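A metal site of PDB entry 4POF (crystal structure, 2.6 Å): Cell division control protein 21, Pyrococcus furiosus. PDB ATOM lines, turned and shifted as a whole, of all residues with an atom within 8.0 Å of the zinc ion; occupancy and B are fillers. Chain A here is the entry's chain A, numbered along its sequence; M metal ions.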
ATOM      1  N   VAL A 139     -21.820  12.320  22.201  1.00  0.00           N
ATOM      2  CA  VAL A 139     -22.151  11.078  21.517  1.00  0.00           C
ATOM      3  C   VAL A 139     -20.903  10.242  21.308  1.00  0.00           C
ATOM      4  O   VAL A 139     -19.855  10.751  20.898  1.00  0.00           O
ATOM      5  CB  VAL A 139     -22.873  11.326  20.176  1.00  0.00           C
ATOM      6  CG1 VAL A 139     -23.182  10.009  19.473  1.00  0.00           C
ATOM      7  CG2 VAL A 139     -24.163  12.098  20.412  1.00  0.00           C
ATOM      8  N   CYS A 140     -21.041   8.960  21.614  1.00  0.00           N
ATOM      9  CA  CYS A 140     -19.992   7.997  21.382  1.00  0.00           C
ATOM     10  C   CYS A 140     -19.826   7.760  19.888  1.00  0.00           C
ATOM     11  O   CYS A 140     -20.738   7.290  19.215  1.00  0.00           O
ATOM     12  CB  CYS A 140     -20.304   6.695  22.108  1.00  0.00           C
ATOM     13  SG  CYS A 140     -19.053   5.415  21.922  1.00  0.00           S
ATOM     14  N   LYS A 141     -18.643   8.094  19.378  1.00  0.00           N
ATOM     15  CA  LYS A 141     -18.291   7.885  17.980  1.00  0.00           C
ATOM     16  C   LYS A 141     -18.279   6.391  17.627  1.00  0.00           C
ATOM     17  O   LYS A 141     -18.446   6.023  16.461  1.00  0.00           O
ATOM     18  CB  LYS A 141     -16.930   8.544  17.693  1.00  0.00           C
ATOM     19  CG  LYS A 141     -16.453   8.505  16.254  1.00  0.00           C
ATOM     20  CD  LYS A 141     -17.010   9.658  15.429  1.00  0.00           C
ATOM     21  CE  LYS A 141     -16.625   9.477  13.966  1.00  0.00           C
ATOM     22  NZ  LYS A 141     -17.232  10.500  13.084  1.00  0.00           N
ATOM     23  N   ASP A 142     -18.111   5.542  18.635  1.00  0.00           N
ATOM     24  CA  ASP A 142     -18.054   4.099  18.418  1.00  0.00           C
ATOM     25  C   ASP A 142     -19.420   3.424  18.548  1.00  0.00           C
ATOM     26  O   ASP A 142     -20.025   3.072  17.530  1.00  0.00           O
ATOM     27  CB  ASP A 142     -16.992   3.455  19.323  1.00  0.00           C
ATOM     28  CG  ASP A 142     -15.581   3.934  19.011  1.00  0.00           C
ATOM     29  OD1 ASP A 142     -14.706   3.845  19.903  1.00  0.00           O
ATOM     30  OD2 ASP A 142     -15.321   4.395  17.877  1.00  0.00           O
ATOM     31  N   CYS A 143     -19.924   3.254  19.773  1.00  0.00           N
ATOM     32  CA  CYS A 143     -21.189   2.527  19.986  1.00  0.00           C
ATOM     33  C   CYS A 143     -22.464   3.381  19.823  1.00  0.00           C
ATOM     34  O   CYS A 143     -23.578   2.861  19.920  1.00  0.00           O
ATOM     35  CB  CYS A 143     -21.209   1.798  21.343  1.00  0.00           C
ATOM     36  SG  CYS A 143     -21.696   2.816  22.741  1.00  0.00           S
ATOM     37  N   GLY A 144     -22.291   4.688  19.614  1.00  0.00           N
ATOM     38  CA  GLY A 144     -23.418   5.587  19.336  1.00  0.00           C
ATOM     39  C   GLY A 144     -24.298   5.965  20.513  1.00  0.00           C
ATOM     40  O   GLY A 144     -25.419   6.452  20.324  1.00  0.00           O
ATOM     41  N   HIS A 145     -23.801   5.758  21.739  1.00  0.00           N
ATOM     42  CA  HIS A 145     -24.551   6.095  22.950  1.00  0.00           C
ATOM     43  C   HIS A 145     -24.503   7.607  23.244  1.00  0.00           C
ATOM     44  O   HIS A 145     -23.492   8.280  23.002  1.00  0.00           O
ATOM     45  CB  HIS A 145     -24.026   5.284  24.152  1.00  0.00           C
ATOM     46  CG  HIS A 145     -24.835   5.478  25.402  1.00  0.00           C
ATOM     47  ND1 HIS A 145     -24.271   5.862  26.597  1.00  0.00           N
ATOM     48  CD2 HIS A 145     -26.155   5.356  25.635  1.00  0.00           C
ATOM     49  CE1 HIS A 145     -25.208   5.964  27.517  1.00  0.00           C
ATOM     50  NE2 HIS A 145     -26.372   5.657  26.957  1.00  0.00           N
ATOM     51  N   GLU A 146     -25.626   8.114  23.756  1.00  0.00           N
ATOM     52  CA  GLU A 146     -25.735   9.537  24.078  1.00  0.00           C
ATOM     53  C   GLU A 146     -25.739   9.799  25.586  1.00  0.00           C
ATOM     54  O   GLU A 146     -26.383   9.090  26.363  1.00  0.00           O
ATOM     55  CB  GLU A 146     -26.983  10.113  23.433  1.00  0.00           C
ATOM     56  CG  GLU A 146     -26.857  10.272  21.926  1.00  0.00           C
ATOM     57  CD  GLU A 146     -28.188  10.518  21.226  1.00  0.00           C
ATOM     58  OE1 GLU A 146     -29.029  11.234  21.788  1.00  0.00           O
ATOM     59  OE2 GLU A 146     -28.373   9.987  20.109  1.00  0.00           O
ATOM     60  N   MET A 147     -25.001  10.830  25.985  1.00  0.00           N
ATOM     61  CA  MET A 147     -24.863  11.228  27.381  1.00  0.00           C
ATOM     62  C   MET A 147     -25.147  12.722  27.597  1.00  0.00           C
ATOM     63  O   MET A 147     -24.550  13.589  26.958  1.00  0.00           O
ATOM     64  CB  MET A 147     -23.458  10.893  27.876  1.00  0.00           C
ATOM     65  CG  MET A 147     -23.080   9.420  27.750  1.00  0.00           C
ATOM     66  SD  MET A 147     -21.293   9.165  27.875  1.00  0.00           S
ATOM     67  CE  MET A 147     -20.999   9.659  29.568  1.00  0.00           C
ATOM     68  N   LYS A 162     -14.553   9.204  28.630  1.00  0.00           N
ATOM     69  CA  LYS A 162     -14.899   7.784  28.609  1.00  0.00           C
ATOM     70  C   LYS A 162     -16.398   7.546  28.414  1.00  0.00           C
ATOM     71  O   LYS A 162     -17.220   8.210  29.032  1.00  0.00           O
ATOM     72  CB  LYS A 162     -14.428   7.092  29.897  1.00  0.00           C
ATOM     73  CG  LYS A 162     -14.497   5.566  29.871  1.00  0.00           C
ATOM     74  CD  LYS A 162     -13.406   4.969  29.007  1.00  0.00           C
ATOM     75  CE  LYS A 162     -12.065   4.939  29.720  1.00  0.00           C
ATOM     76  NZ  LYS A 162     -12.134   4.051  30.909  1.00  0.00           N
ATOM     77  N   CYS A 163     -16.733   6.580  27.556  1.00  0.00           N
ATOM     78  CA  CYS A 163     -18.127   6.197  27.316  1.00  0.00           C
ATOM     79  C   CYS A 163     -18.729   5.424  28.497  1.00  0.00           C
ATOM     80  O   CYS A 163     -18.180   4.407  28.932  1.00  0.00           O
ATOM     81  CB  CYS A 163     -18.229   5.360  26.041  1.00  0.00           C
ATOM     82  SG  CYS A 163     -19.893   4.896  25.549  1.00  0.00           S
ATOM     83  N   GLU A 164     -19.850   5.929  28.996  1.00  0.00           N
ATOM     84  CA  GLU A 164     -20.555   5.384  30.170  1.00  0.00           C
ATOM     85  C   GLU A 164     -21.108   3.962  29.964  1.00  0.00           C
ATOM     86  O   GLU A 164     -21.431   3.270  30.927  1.00  0.00           O
ATOM     87  CB  GLU A 164     -21.657   6.378  30.562  1.00  0.00           C
ATOM     88  CG  GLU A 164     -22.687   5.924  31.590  1.00  0.00           C
ATOM     89  CD  GLU A 164     -23.917   6.826  31.601  1.00  0.00           C
ATOM     90  OE1 GLU A 164     -24.977   6.393  32.097  1.00  0.00           O
ATOM     91  OE2 GLU A 164     -23.824   7.976  31.109  1.00  0.00           O
ATOM     92  N   GLN A 165     -21.176   3.534  28.709  1.00  0.00           N
ATOM     93  CA  GLN A 165     -21.770   2.242  28.364  1.00  0.00           C
ATOM     94  C   GLN A 165     -20.770   1.210  27.840  1.00  0.00           C
ATOM     95  O   GLN A 165     -20.624   0.135  28.420  1.00  0.00           O
ATOM     96  CB  GLN A 165     -22.915   2.430  27.383  1.00  0.00           C
ATOM     97  CG  GLN A 165     -23.733   1.187  27.148  1.00  0.00           C
ATOM     98  CD  GLN A 165     -24.846   1.412  26.151  1.00  0.00           C
ATOM     99  OE1 GLN A 165     -24.599   1.758  24.992  1.00  0.00           O
ATOM    100  NE2 GLN A 165     -26.079   1.221  26.591  1.00  0.00           N
ATOM    101  N   CYS A 166     -20.094   1.534  26.730  1.00  0.00           N
ATOM    102  CA  CYS A 166     -19.110   0.623  26.138  1.00  0.00           C
ATOM    103  C   CYS A 166     -17.674   0.890  26.601  1.00  0.00           C
ATOM    104  O   CYS A 166     -16.816   0.009  26.500  1.00  0.00           O
ATOM    105  CB  CYS A 166     -19.198   0.646  24.608  1.00  0.00           C
ATOM    106  SG  CYS A 166     -18.288   2.000  23.820  1.00  0.00           S
ATOM    107  N   GLY A 167     -17.421   2.092  27.099  1.00  0.00           N
ATOM    108  CA  GLY A 167     -16.098   2.464  27.606  1.00  0.00           C
ATOM    109  C   GLY A 167     -15.053   2.750  26.552  1.00  0.00           C
ATOM    110  O   GLY A 167     -13.874   2.498  26.765  1.00  0.00           O
ATOM    111  N   SER A 168     -15.476   3.291  25.401  1.00  0.00           N
ATOM    112  CA  SER A 168     -14.552   3.707  24.356  1.00  0.00           C
ATOM    113  C   SER A 168     -14.130   5.162  24.543  1.00  0.00           C
ATOM    114  O   SER A 168     -14.910   5.977  25.046  1.00  0.00           O
ATOM    115  CB  SER A 168     -15.162   3.517  22.981  1.00  0.00           C
ATOM    116  OG  SER A 168     -16.342   4.278  22.836  1.00  0.00           O
ATOM    117  N   LYS A 169     -12.912   5.479  24.121  1.00  0.00           N
ATOM    118  CA  LYS A 169     -12.339   6.832  24.284  1.00  0.00           C
ATOM    119  C   LYS A 169     -12.512   7.701  23.039  1.00  0.00           C
ATOM    120  O   LYS A 169     -11.795   8.678  22.835  1.00  0.00           O
ATOM    121  CB  LYS A 169     -10.857   6.751  24.687  1.00  0.00           C
ATOM    122  CG  LYS A 169     -10.639   6.286  26.106  1.00  0.00           C
ATOM    123  CD  LYS A 169      -9.178   6.322  26.470  1.00  0.00           C
ATOM    124  CE  LYS A 169      -8.961   5.879  27.899  1.00  0.00           C
ATOM    125  NZ  LYS A 169      -7.520   5.922  28.302  1.00  0.00           N
ATOM    126  N   ASN A 170     -13.500   7.340  22.218  1.00  0.00           N
ATOM    127  CA  ASN A 170     -13.816   8.077  20.997  1.00  0.00           C
ATOM    128  C   ASN A 170     -15.187   8.760  21.105  1.00  0.00           C
ATOM    129  O   ASN A 170     -16.205   8.206  20.685  1.00  0.00           O
ATOM    130  CB  ASN A 170     -13.760   7.125  19.797  1.00  0.00           C
ATOM    131  CG  ASN A 170     -13.337   7.828  18.521  1.00  0.00           C
ATOM    132  OD1 ASN A 170     -13.598   9.025  18.322  1.00  0.00           O
ATOM    133  ND2 ASN A 170     -12.682   7.085  17.637  1.00  0.00           N
ATOM    134  N   ILE A 171     -15.195   9.966  21.671  1.00  0.00           N
ATOM    135  CA  ILE A 171     -16.426  10.711  21.942  1.00  0.00           C
ATOM    136  C   ILE A 171     -16.329  12.138  21.408  1.00  0.00           C
ATOM    137  O   ILE A 171     -15.245  12.721  21.375  1.00  0.00           O
ATOM    138  CB  ILE A 171     -16.745  10.779  23.473  1.00  0.00           C
ATOM    139  CG1 ILE A 171     -16.378   9.477  24.208  1.00  0.00           C
ATOM    140  CG2 ILE A 171     -18.193  11.215  23.723  1.00  0.00           C
ATOM    141  CD1 ILE A 171     -17.268   8.275  23.896  1.00  0.00           C
HETATM  142 ZN    ZN M   1     -19.728   3.814  23.459  1.00  0.00          ZN
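The zinc ion is bound by SG of Cys 140 (2.3 Å). The side-chain sulfur (SG) of Cys 143 is bound to the zinc ion (2.3 Å). SG of Cys 166 binds the zinc ion (2.3 Å). SG of Cys 163 binds the zinc ion (2.4 Å).
The backbone NH of Asp 142 sits close to the side-chain sulfur of Cys 140 (3.4 Å). The side-chain hydroxyl (OG) of Ser 168 lies close to the side-chain sulfur (SG) of Cys 140, 3.1 Å away. The side-chain hydroxyl (OG) of Ser 168 sits close to the side-chain sulfur (SG) of Cys 166, at 3.2 Å. O of His 145 is in hydrogen-bond range of N of Cys 140, 2.9 Å away. O of Ser 168 lies within hydrogen-bond range of N of Cys 163. N of Gln 165 lies close to SG of Cys 163 (3.7 Å). OD1 of Asp 142 lies close to OG of Ser 168 (3.4 Å). The side-chain sulfur (SG) of Cys 143 sits close to the backbone NH (N) of His 145 (3.8 Å).
Ser 168 touches the zinc ion (OG to ZN, 3.5 Å). Of the 19 residues printed, 5 come within 4 Å of the zinc ion. Along chain A the residues within 4 Å of the zinc ion span positions 140 to 168. The nearest printed residue that does not touch the zinc ion is His 145 (4.6 Å).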
